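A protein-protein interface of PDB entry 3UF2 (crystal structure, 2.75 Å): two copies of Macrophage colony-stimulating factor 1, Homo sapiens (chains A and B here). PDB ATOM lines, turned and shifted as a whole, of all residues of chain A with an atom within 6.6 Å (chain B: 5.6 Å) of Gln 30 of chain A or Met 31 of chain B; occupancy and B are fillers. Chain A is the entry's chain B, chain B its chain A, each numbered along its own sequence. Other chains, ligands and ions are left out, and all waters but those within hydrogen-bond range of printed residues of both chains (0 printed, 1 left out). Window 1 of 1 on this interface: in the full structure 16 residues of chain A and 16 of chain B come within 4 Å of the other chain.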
ATOM      1  N   ARG A  25      18.185 -21.278 -11.622  1.00  0.00           N
ATOM      2  CA  ARG A  25      16.998 -20.532 -12.020  1.00  0.00           C
ATOM      3  C   ARG A  25      16.294 -21.244 -13.169  1.00  0.00           C
ATOM      4  O   ARG A  25      15.068 -21.372 -13.171  1.00  0.00           O
ATOM      5  CB  ARG A  25      17.357 -19.102 -12.430  1.00  0.00           C
ATOM      6  CG  ARG A  25      17.717 -18.190 -11.264  1.00  0.00           C
ATOM      7  CD  ARG A  25      17.764 -16.734 -11.696  1.00  0.00           C
ATOM      8  NE  ARG A  25      16.428 -16.136 -11.738  1.00  0.00           N
ATOM      9  CZ  ARG A  25      15.942 -15.408 -12.743  1.00  0.00           C
ATOM     10  NH1 ARG A  25      14.710 -14.924 -12.662  1.00  0.00           N
ATOM     11  NH2 ARG A  25      16.664 -15.159 -13.829  1.00  0.00           N
ATOM     12  N   LEU A  26      17.073 -21.710 -14.138  1.00  0.00           N
ATOM     13  CA  LEU A  26      16.526 -22.423 -15.281  1.00  0.00           C
ATOM     14  C   LEU A  26      15.843 -23.701 -14.810  1.00  0.00           C
ATOM     15  O   LEU A  26      14.742 -24.028 -15.248  1.00  0.00           O
ATOM     16  CB  LEU A  26      17.638 -22.738 -16.283  1.00  0.00           C
ATOM     17  CG  LEU A  26      17.205 -23.320 -17.627  1.00  0.00           C
ATOM     18  CD1 LEU A  26      18.169 -22.881 -18.716  1.00  0.00           C
ATOM     19  CD2 LEU A  26      17.135 -24.836 -17.556  1.00  0.00           C
ATOM     20  N   ILE A  27      16.499 -24.411 -13.899  1.00  0.00           N
ATOM     21  CA  ILE A  27      15.947 -25.636 -13.334  1.00  0.00           C
ATOM     22  C   ILE A  27      14.677 -25.349 -12.531  1.00  0.00           C
ATOM     23  O   ILE A  27      13.738 -26.145 -12.532  1.00  0.00           O
ATOM     24  CB  ILE A  27      16.982 -26.331 -12.429  1.00  0.00           C
ATOM     25  CG1 ILE A  27      18.176 -26.799 -13.262  1.00  0.00           C
ATOM     26  CG2 ILE A  27      16.360 -27.516 -11.702  1.00  0.00           C
ATOM     27  CD1 ILE A  27      19.369 -27.212 -12.435  1.00  0.00           C
ATOM     28  N   ASP A  28      14.649 -24.204 -11.856  1.00  0.00           N
ATOM     29  CA  ASP A  28      13.512 -23.833 -11.016  1.00  0.00           C
ATOM     30  C   ASP A  28      12.340 -23.321 -11.849  1.00  0.00           C
ATOM     31  O   ASP A  28      11.215 -23.230 -11.356  1.00  0.00           O
ATOM     32  CB  ASP A  28      13.919 -22.754 -10.007  1.00  0.00           C
ATOM     33  CG  ASP A  28      15.016 -23.212  -9.062  1.00  0.00           C
ATOM     34  OD1 ASP A  28      15.154 -24.436  -8.848  1.00  0.00           O
ATOM     35  OD2 ASP A  28      15.740 -22.343  -8.534  1.00  0.00           O
ATOM     36  N   SER A  29      12.608 -22.981 -13.106  1.00  0.00           N
ATOM     37  CA  SER A  29      11.586 -22.418 -13.983  1.00  0.00           C
ATOM     38  C   SER A  29      10.828 -23.490 -14.763  1.00  0.00           C
ATOM     39  O   SER A  29       9.718 -23.248 -15.237  1.00  0.00           O
ATOM     40  CB  SER A  29      12.217 -21.426 -14.962  1.00  0.00           C
ATOM     41  OG  SER A  29      13.172 -22.061 -15.793  1.00  0.00           O
ATOM     42  N   GLN A  30      11.423 -24.671 -14.894  1.00  0.00           N
ATOM     43  CA  GLN A  30      10.819 -25.745 -15.677  1.00  0.00           C
ATOM     44  C   GLN A  30       9.643 -26.395 -14.948  1.00  0.00           C
ATOM     45  O   GLN A  30       9.667 -26.566 -13.728  1.00  0.00           O
ATOM     46  CB  GLN A  30      11.868 -26.800 -16.034  1.00  0.00           C
ATOM     47  CG  GLN A  30      13.026 -26.255 -16.854  1.00  0.00           C
ATOM     48  CD  GLN A  30      12.565 -25.518 -18.099  1.00  0.00           C
ATOM     49  OE1 GLN A  30      11.927 -26.099 -18.974  1.00  0.00           O
ATOM     50  NE2 GLN A  30      12.879 -24.230 -18.178  1.00  0.00           N
ATOM     51  N   MET A  31       8.620 -26.759 -15.717  1.00  0.00           N
ATOM     52  CA  MET A  31       7.393 -27.325 -15.168  1.00  0.00           C
ATOM     53  C   MET A  31       7.596 -28.775 -14.741  1.00  0.00           C
ATOM     54  O   MET A  31       8.288 -29.541 -15.412  1.00  0.00           O
ATOM     55  CB  MET A  31       6.275 -27.238 -16.208  1.00  0.00           C
ATOM     56  CG  MET A  31       4.893 -27.573 -15.671  1.00  0.00           C
ATOM     57  SD  MET A  31       3.575 -26.964 -16.741  1.00  0.00           S
ATOM     58  CE  MET A  31       3.738 -28.055 -18.150  1.00  0.00           C
ATOM     59  N   GLU A  32       6.987 -29.145 -13.618  1.00  0.00           N
ATOM     60  CA  GLU A  32       7.106 -30.500 -13.092  1.00  0.00           C
ATOM     61  C   GLU A  32       6.034 -31.407 -13.687  1.00  0.00           C
ATOM     62  O   GLU A  32       4.883 -31.394 -13.249  1.00  0.00           O
ATOM     63  CB  GLU A  32       6.994 -30.492 -11.566  1.00  0.00           C
ATOM     64  CG  GLU A  32       8.049 -29.650 -10.867  1.00  0.00           C
ATOM     65  CD  GLU A  32       7.963 -29.755  -9.355  1.00  0.00           C
ATOM     66  OE1 GLU A  32       8.936 -29.368  -8.674  1.00  0.00           O
ATOM     67  OE2 GLU A  32       6.924 -30.225  -8.846  1.00  0.00           O
ATOM     68  N   THR A  33       6.422 -32.195 -14.683  1.00  0.00           N
ATOM     69  CA  THR A  33       5.486 -33.079 -15.367  1.00  0.00           C
ATOM     70  C   THR A  33       6.023 -34.506 -15.424  1.00  0.00           C
ATOM     71  O   THR A  33       7.086 -34.805 -14.879  1.00  0.00           O
ATOM     72  CB  THR A  33       5.208 -32.601 -16.811  1.00  0.00           C
ATOM     73  OG1 THR A  33       6.397 -32.724 -17.600  1.00  0.00           O
ATOM     74  CG2 THR A  33       4.747 -31.156 -16.828  1.00  0.00           C
ATOM     75  N   ILE A  37      12.187 -37.424 -21.912  1.00  0.00           N
ATOM     76  CA  ILE A  37      12.882 -37.173 -23.169  1.00  0.00           C
ATOM     77  C   ILE A  37      14.069 -38.113 -23.337  1.00  0.00           C
ATOM     78  O   ILE A  37      14.457 -38.815 -22.401  1.00  0.00           O
ATOM     79  CB  ILE A  37      13.382 -35.719 -23.257  1.00  0.00           C
ATOM     80  CG1 ILE A  37      14.248 -35.374 -22.042  1.00  0.00           C
ATOM     81  CG2 ILE A  37      12.205 -34.765 -23.352  1.00  0.00           C
ATOM     82  CD1 ILE A  37      14.937 -34.026 -22.143  1.00  0.00           C
ATOM     83  N   THR A  68      19.496 -30.575 -27.264  1.00  0.00           N
ATOM     84  CA  THR A  68      18.295 -30.841 -26.478  1.00  0.00           C
ATOM     85  C   THR A  68      17.776 -29.614 -25.726  1.00  0.00           C
ATOM     86  O   THR A  68      16.579 -29.330 -25.749  1.00  0.00           O
ATOM     87  CB  THR A  68      18.544 -31.976 -25.467  1.00  0.00           C
ATOM     88  OG1 THR A  68      18.984 -33.147 -26.166  1.00  0.00           O
ATOM     89  CG2 THR A  68      17.273 -32.298 -24.686  1.00  0.00           C
ATOM     90  N   MET A  69      18.672 -28.895 -25.057  1.00  0.00           N
ATOM     91  CA  MET A  69      18.272 -27.763 -24.229  1.00  0.00           C
ATOM     92  C   MET A  69      18.074 -26.508 -25.072  1.00  0.00           C
ATOM     93  O   MET A  69      18.969 -25.666 -25.173  1.00  0.00           O
ATOM     94  CB  MET A  69      19.315 -27.513 -23.137  1.00  0.00           C
ATOM     95  CG  MET A  69      19.456 -28.673 -22.159  1.00  0.00           C
ATOM     96  SD  MET A  69      20.849 -28.518 -21.026  1.00  0.00           S
ATOM     97  CE  MET A  69      20.464 -26.960 -20.240  1.00  0.00           C
ATOM     98  N   ARG A  70      16.892 -26.387 -25.669  1.00  0.00           N
ATOM     99  CA  ARG A  70      16.576 -25.262 -26.542  1.00  0.00           C
ATOM    100  C   ARG A  70      15.408 -24.462 -25.978  1.00  0.00           C
ATOM    101  O   ARG A  70      14.383 -25.026 -25.598  1.00  0.00           O
ATOM    102  CB  ARG A  70      16.244 -25.764 -27.948  1.00  0.00           C
ATOM    103  CG  ARG A  70      17.175 -26.870 -28.426  1.00  0.00           C
ATOM    104  CD  ARG A  70      17.066 -27.126 -29.921  1.00  0.00           C
ATOM    105  NE  ARG A  70      15.875 -27.900 -30.279  1.00  0.00           N
ATOM    106  CZ  ARG A  70      14.859 -27.454 -31.019  1.00  0.00           C
ATOM    107  NH1 ARG A  70      14.850 -26.219 -31.511  1.00  0.00           N
ATOM    108  NH2 ARG A  70      13.835 -28.258 -31.275  1.00  0.00           N
ATOM    109  N   PHE A  71      15.573 -23.144 -25.920  1.00  0.00           N
ATOM    110  CA  PHE A  71      14.543 -22.260 -25.385  1.00  0.00           C
ATOM    111  C   PHE A  71      14.262 -21.123 -26.359  1.00  0.00           C
ATOM    112  O   PHE A  71      15.143 -20.722 -27.119  1.00  0.00           O
ATOM    113  CB  PHE A  71      14.985 -21.694 -24.035  1.00  0.00           C
ATOM    114  CG  PHE A  71      15.282 -22.745 -23.009  1.00  0.00           C
ATOM    115  CD1 PHE A  71      16.526 -23.349 -22.954  1.00  0.00           C
ATOM    116  CD2 PHE A  71      14.313 -23.138 -22.103  1.00  0.00           C
ATOM    117  CE1 PHE A  71      16.800 -24.322 -22.014  1.00  0.00           C
ATOM    118  CE2 PHE A  71      14.581 -24.109 -21.161  1.00  0.00           C
ATOM    119  CZ  PHE A  71      15.825 -24.702 -21.117  1.00  0.00           C
ATOM    120  N   ASN A  77      16.438 -17.975 -20.056  1.00  0.00           N
ATOM    121  CA  ASN A  77      16.991 -19.322 -20.131  1.00  0.00           C
ATOM    122  C   ASN A  77      17.804 -19.542 -21.407  1.00  0.00           C
ATOM    123  O   ASN A  77      18.867 -20.158 -21.366  1.00  0.00           O
ATOM    124  CB  ASN A  77      15.877 -20.369 -20.019  1.00  0.00           C
ATOM    125  CG  ASN A  77      15.290 -20.454 -18.616  1.00  0.00           C
ATOM    126  OD1 ASN A  77      15.920 -20.045 -17.640  1.00  0.00           O
ATOM    127  ND2 ASN A  77      14.080 -20.997 -18.510  1.00  0.00           N
ATOM    128  N   PRO A 114      13.038 -33.940 -18.248  1.00  0.00           N
ATOM    129  CA  PRO A 114      13.926 -32.793 -18.447  1.00  0.00           C
ATOM    130  C   PRO A 114      14.575 -32.341 -17.138  1.00  0.00           C
ATOM    131  O   PRO A 114      15.685 -31.811 -17.155  1.00  0.00           O
ATOM    132  CB  PRO A 114      12.982 -31.716 -18.986  1.00  0.00           C
ATOM    133  CG  PRO A 114      11.916 -32.480 -19.692  1.00  0.00           C
ATOM    134  CD  PRO A 114      11.724 -33.737 -18.884  1.00  0.00           C
ATOM    135  N   LEU A 115      13.891 -32.555 -16.018  1.00  0.00           N
ATOM    136  CA  LEU A 115      14.430 -32.177 -14.715  1.00  0.00           C
ATOM    137  C   LEU A 115      15.555 -33.114 -14.285  1.00  0.00           C
ATOM    138  O   LEU A 115      16.585 -32.666 -13.777  1.00  0.00           O
ATOM    139  CB  LEU A 115      13.324 -32.156 -13.659  1.00  0.00           C
ATOM    140  CG  LEU A 115      12.406 -30.932 -13.704  1.00  0.00           C
ATOM    141  CD1 LEU A 115      11.262 -31.086 -12.718  1.00  0.00           C
ATOM    142  CD2 LEU A 115      13.187 -29.658 -13.413  1.00  0.00           C
ATOM    143  N   LEU A 117      17.401 -34.705 -16.301  1.00  0.00           N
ATOM    144  CA  LEU A 117      18.494 -34.339 -17.190  1.00  0.00           C
ATOM    145  C   LEU A 117      19.244 -33.128 -16.646  1.00  0.00           C
ATOM    146  O   LEU A 117      20.429 -33.213 -16.330  1.00  0.00           O
ATOM    147  CB  LEU A 117      17.962 -34.032 -18.590  1.00  0.00           C
ATOM    148  CG  LEU A 117      18.979 -33.423 -19.558  1.00  0.00           C
ATOM    149  CD1 LEU A 117      20.155 -34.365 -19.761  1.00  0.00           C
ATOM    150  CD2 LEU A 117      18.329 -33.081 -20.889  1.00  0.00           C
ATOM    151  N   LEU A 118      18.546 -32.002 -16.532  1.00  0.00           N
ATOM    152  CA  LEU A 118      19.169 -30.750 -16.109  1.00  0.00           C
ATOM    153  C   LEU A 118      19.974 -30.920 -14.825  1.00  0.00           C
ATOM    154  O   LEU A 118      20.979 -30.239 -14.620  1.00  0.00           O
ATOM    155  CB  LEU A 118      18.108 -29.665 -15.921  1.00  0.00           C
ATOM    156  CG  LEU A 118      17.424 -29.192 -17.207  1.00  0.00           C
ATOM    157  CD1 LEU A 118      16.245 -28.279 -16.895  1.00  0.00           C
ATOM    158  CD2 LEU A 118      18.418 -28.486 -18.108  1.00  0.00           C
ATOM    159  N   SER B  29       9.451 -19.679 -20.906  1.00  0.00           N
ATOM    160  CA  SER B  29      10.511 -20.152 -20.022  1.00  0.00           C
ATOM    161  C   SER B  29      10.675 -21.666 -20.073  1.00  0.00           C
ATOM    162  O   SER B  29      11.698 -22.203 -19.642  1.00  0.00           O
ATOM    163  CB  SER B  29      10.231 -19.717 -18.580  1.00  0.00           C
ATOM    164  OG  SER B  29       8.981 -20.207 -18.121  1.00  0.00           O
ATOM    165  N   GLN B  30       9.666 -22.354 -20.597  1.00  0.00           N
ATOM    166  CA  GLN B  30       9.699 -23.808 -20.664  1.00  0.00           C
ATOM    167  C   GLN B  30      10.624 -24.274 -21.777  1.00  0.00           C
ATOM    168  O   GLN B  30      10.759 -23.611 -22.805  1.00  0.00           O
ATOM    169  CB  GLN B  30       8.294 -24.366 -20.889  1.00  0.00           C
ATOM    170  CG  GLN B  30       7.330 -24.044 -19.770  1.00  0.00           C
ATOM    171  CD  GLN B  30       7.892 -24.406 -18.413  1.00  0.00           C
ATOM    172  OE1 GLN B  30       8.122 -25.579 -18.117  1.00  0.00           O
ATOM    173  NE2 GLN B  30       8.134 -23.396 -17.585  1.00  0.00           N
ATOM    174  N   MET B  31      11.262 -25.419 -21.560  1.00  0.00           N
ATOM    175  CA  MET B  31      12.158 -25.995 -22.549  1.00  0.00           C
ATOM    176  C   MET B  31      11.329 -26.676 -23.629  1.00  0.00           C
ATOM    177  O   MET B  31      10.358 -27.372 -23.334  1.00  0.00           O
ATOM    178  CB  MET B  31      13.104 -27.000 -21.891  1.00  0.00           C
ATOM    179  CG  MET B  31      14.316 -27.361 -22.736  1.00  0.00           C
ATOM    180  SD  MET B  31      15.517 -28.369 -21.843  1.00  0.00           S
ATOM    181  CE  MET B  31      14.596 -29.888 -21.649  1.00  0.00           C
ATOM    182  N   GLU B  32      11.717 -26.464 -24.882  1.00  0.00           N
ATOM    183  CA  GLU B  32      10.986 -27.007 -26.016  1.00  0.00           C
ATOM    184  C   GLU B  32      11.352 -28.474 -26.209  1.00  0.00           C
ATOM    185  O   GLU B  32      12.461 -28.795 -26.634  1.00  0.00           O
ATOM    186  CB  GLU B  32      11.309 -26.204 -27.276  1.00  0.00           C
ATOM    187  CG  GLU B  32      11.101 -24.703 -27.106  1.00  0.00           C
ATOM    188  CD  GLU B  32      11.573 -23.900 -28.302  1.00  0.00           C
ATOM    189  OE1 GLU B  32      11.342 -22.673 -28.320  1.00  0.00           O
ATOM    190  OE2 GLU B  32      12.178 -24.492 -29.219  1.00  0.00           O
ATOM    191  N   THR B  33      10.413 -29.360 -25.890  1.00  0.00           N
ATOM    192  CA  THR B  33      10.679 -30.794 -25.899  1.00  0.00           C
ATOM    193  C   THR B  33       9.718 -31.552 -26.811  1.00  0.00           C
ATOM    194  O   THR B  33       8.645 -31.058 -27.156  1.00  0.00           O
ATOM    195  CB  THR B  33      10.571 -31.381 -24.482  1.00  0.00           C
ATOM    196  OG1 THR B  33       9.267 -31.114 -23.950  1.00  0.00           O
ATOM    197  CG2 THR B  33      11.622 -30.767 -23.569  1.00  0.00           C
ATOM    198  N   ARG B  70       2.588 -27.863 -12.215  1.00  0.00           N
ATOM    199  CA  ARG B  70       3.212 -27.690 -10.907  1.00  0.00           C
ATOM    200  C   ARG B  70       4.642 -27.188 -11.037  1.00  0.00           C
ATOM    201  O   ARG B  70       5.429 -27.723 -11.818  1.00  0.00           O
ATOM    202  CB  ARG B  70       3.212 -29.008 -10.129  1.00  0.00           C
ATOM    203  CG  ARG B  70       1.830 -29.515  -9.748  1.00  0.00           C
ATOM    204  CD  ARG B  70       1.916 -30.757  -8.872  1.00  0.00           C
ATOM    205  NE  ARG B  70       2.691 -31.824  -9.505  1.00  0.00           N
ATOM    206  CZ  ARG B  70       3.992 -32.041  -9.313  1.00  0.00           C
ATOM    207  NH1 ARG B  70       4.701 -31.274  -8.494  1.00  0.00           N
ATOM    208  NH2 ARG B  70       4.591 -33.041  -9.944  1.00  0.00           N
ATOM    209  N   PHE B  71       4.972 -26.163 -10.256  1.00  0.00           N
ATOM    210  CA  PHE B  71       6.315 -25.592 -10.255  1.00  0.00           C
ATOM    211  C   PHE B  71       6.904 -25.617  -8.853  1.00  0.00           C
ATOM    212  O   PHE B  71       6.173 -25.690  -7.865  1.00  0.00           O
ATOM    213  CB  PHE B  71       6.282 -24.160 -10.785  1.00  0.00           C
ATOM    214  CG  PHE B  71       5.812 -24.056 -12.205  1.00  0.00           C
ATOM    215  CD1 PHE B  71       4.462 -23.949 -12.496  1.00  0.00           C
ATOM    216  CD2 PHE B  71       6.719 -24.079 -13.250  1.00  0.00           C
ATOM    217  CE1 PHE B  71       4.027 -23.861 -13.803  1.00  0.00           C
ATOM    218  CE2 PHE B  71       6.289 -23.991 -14.558  1.00  0.00           C
ATOM    219  CZ  PHE B  71       4.942 -23.883 -14.836  1.00  0.00           C
ATOM    220  N   ARG B  72       8.229 -25.562  -8.774  1.00  0.00           N
ATOM    221  CA  ARG B  72       8.917 -25.553  -7.491  1.00  0.00           C
ATOM    222  C   ARG B  72       8.416 -24.381  -6.657  1.00  0.00           C
ATOM    223  O   ARG B  72       8.211 -23.283  -7.174  1.00  0.00           O
ATOM    224  CB  ARG B  72      10.429 -25.448  -7.695  1.00  0.00           C
ATOM    225  CG  ARG B  72      11.235 -25.648  -6.424  1.00  0.00           C
ATOM    226  CD  ARG B  72      12.716 -25.407  -6.656  1.00  0.00           C
ATOM    227  NE  ARG B  72      13.485 -25.539  -5.421  1.00  0.00           N
ATOM    228  CZ  ARG B  72      13.550 -24.609  -4.473  1.00  0.00           C
ATOM    229  NH1 ARG B  72      12.887 -23.465  -4.603  1.00  0.00           N
ATOM    230  NH2 ARG B  72      14.276 -24.822  -3.384  1.00  0.00           N
ATOM    231  N   ASN B  77       7.050 -18.691 -11.495  1.00  0.00           N
ATOM    232  CA  ASN B  77       6.020 -19.465 -12.181  1.00  0.00           C
ATOM    233  C   ASN B  77       5.010 -20.080 -11.219  1.00  0.00           C
ATOM    234  O   ASN B  77       3.823 -20.166 -11.529  1.00  0.00           O
ATOM    235  CB  ASN B  77       6.656 -20.561 -13.035  1.00  0.00           C
ATOM    236  CG  ASN B  77       7.367 -20.009 -14.254  1.00  0.00           C
ATOM    237  OD1 ASN B  77       6.993 -18.960 -14.781  1.00  0.00           O
ATOM    238  ND2 ASN B  77       8.398 -20.714 -14.711  1.00  0.00           N
ATOM    239  N   LEU B 115       4.007 -27.629 -23.853  1.00  0.00           N
ATOM    240  CA  LEU B 115       3.780 -26.297 -24.406  1.00  0.00           C
ATOM    241  C   LEU B 115       2.422 -26.212 -25.098  1.00  0.00           C
ATOM    242  O   LEU B 115       1.729 -25.200 -24.999  1.00  0.00           O
ATOM    243  CB  LEU B 115       4.904 -25.918 -25.372  1.00  0.00           C
ATOM    244  CG  LEU B 115       6.237 -25.583 -24.693  1.00  0.00           C
ATOM    245  CD1 LEU B 115       7.403 -25.726 -25.661  1.00  0.00           C
ATOM    246  CD2 LEU B 115       6.200 -24.177 -24.116  1.00  0.00           C
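Ser 29 of chain A touches Phe 71 of chain B, and with the chains exchanged Phe 71 of chain A touches Ser 29 of chain B.
Gln 30 of chain A touches Met 31 of chain B, and with the chains exchanged Met 31 of chain A touches Gln 30 of chain B.
Gln 30 of chain A touches Phe 71 of chain B, and with the chains exchanged Phe 71 of chain A touches Gln 30 of chain B.
Glu 32 of chain A touches Arg 70 of chain B, and with the chains exchanged Arg 70 of chain A touches Glu 32 of chain B.
Printed residues of chain B within 4 Å of Ser 29 of chain A: Gln 30 (2.8 Å), Phe 71 (3.6 Å) and Asn 77 (2.9 Å).
Thr 68 of chain A touches none of the printed residues of chain B.
Of the printed residues of chain B, Asn 77 of chain A touches Ser 29 (2.9 Å).
Of the printed residues of chain A, Gln 30 of chain B touches Ser 29, Gln 30, Met 31 and Phe 71.
Met 31 of chain B touches five residues of chain A.
Of the printed residues of chain A, Arg 70 of chain B touches Met 31 (3.8 Å) and Glu 32 (2.5 Å).
Printed residues of chain A within 4 Å of Phe 71 of chain B: Ser 29 (3.6 Å), Gln 30 (3.9 Å) and Met 31 (3.6 Å).
The nearest residue of chain B that does not touch Gln 30 of chain A is Arg 70 of chain B (4.8 Å).
The nearest printed residue of chain B that does not touch Arg 70 of chain A is Gln 30 of chain B (4.8 Å).
The backbone carbonyl oxygen (O) of Ser 29 of chain B sits at hydrogen-bond distance from the side-chain amide nitrogen (NE2) of Gln 30 of chain A, 2.8 Å away.
The backbone carbonyl oxygen (O) of Ser 29 of chain B sits at hydrogen-bond distance from the side-chain amide nitrogen (ND2) of Asn 77 of chain A, 2.9 Å away.
NE2 of Gln 30 of chain B lies within hydrogen-bond range of O of Ser 29 of chain A.
N of Met 31 of chain A sits at hydrogen-bond distance from OE1 of Gln 30 of chain B (2.7 Å).
The backbone NH of Met 31 of chain B sits at hydrogen-bond distance from the side-chain amide oxygen of Gln 30 of chain A, 2.8 Å away.
NH1 of Arg 70 of chain A lies within salt-bridge range of OE2 of Glu 32 of chain B (3.9 Å).
The side-chain carboxylate (OE2) of Glu 32 of chain A lies within salt-bridge range of the guanidinium group (NH1) of Arg 70 of chain B, 2.5 Å away.
NE of Arg 72 of chain B is in salt-bridge range of OD1 of Asp 28 of chain A (3.97 Å).
The side-chain amide nitrogen (ND2) of Asn 77 of chain B lies within hydrogen-bond range of the backbone carbonyl oxygen (O) of Ser 29 of chain A (2.9 Å).
The side-chain hydroxyl (OG) of Ser 29 of chain A lies within hydrogen-bond range of the backbone carbonyl oxygen (O) of Arg 25 of chain A (3.3 Å).
The side-chain hydroxyl (OG) of Ser 29 of chain A lies within hydrogen-bond range of the backbone carbonyl oxygen (O) of Leu 26 of chain A (2.6 Å).
The backbone carbonyl oxygen of Leu 26 of chain A sits close to the side-chain amide nitrogen of Gln 30 of chain A, at 3.5 Å.
The side-chain hydroxyl (OG) of Ser 29 of chain A is in hydrogen-bond range of the side-chain amide nitrogen (NE2) of Gln 30 of chain A (3.2 Å).
The side-chain hydroxyl (OG) of Ser 29 of chain A sits at hydrogen-bond distance from the side-chain amide nitrogen (ND2) of Asn 77 of chain A (3.1 Å).
NE2 of Gln 30 of chain A sits close to ND2 of Asn 77 of chain A.
Ser 29 of chain A touches Phe 71 of chain B (O to CE2, 3.6 Å).
C of Met 31 of chain A touches O of Arg 70 of chain B, 3.8 Å away.
Met 31 of chain A touches Phe 71 of chain B (CA to CE2, 3.6 Å).
SD of Met 31 of chain B touches CA of Met 69 of chain A, at 3.7 Å.
Arg 70 of chain A touches Met 31 of chain B (O to CG, 3.7 Å).
Phe 71 of chain A touches Ser 29 of chain B (CD2 to O, 3.7 Å).
Gln 30 of chain B touches Phe 71 of chain A.
Phe 71 of chain A touches Met 31 of chain B.
Glu 32 of chain B touches Phe 71 of chain A.
Pro 114 of chain A touches Met 31 of chain B (CB to CE, 3.6 Å).
Printed residues of chain B that touch a printed residue of chain A: Ser 29, Gln 30, Met 31, Glu 32, Thr 33, Arg 70, Phe 71, Arg 72 and Asn 77.
Among the printed residues, 23 pairs touch across the chains.
Among the printed residues, Asp or Glu carboxylates within 4 Å of a Lys or Arg side-chain nitrogen of the other chain: Asp 28 of chain A with Arg 72 of chain B (3.97 Å), Glu 32 of chain A with Arg 70 of chain B (2.5 Å) and Arg 70 of chain A with Glu 32 of chain B (3.9 Å).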
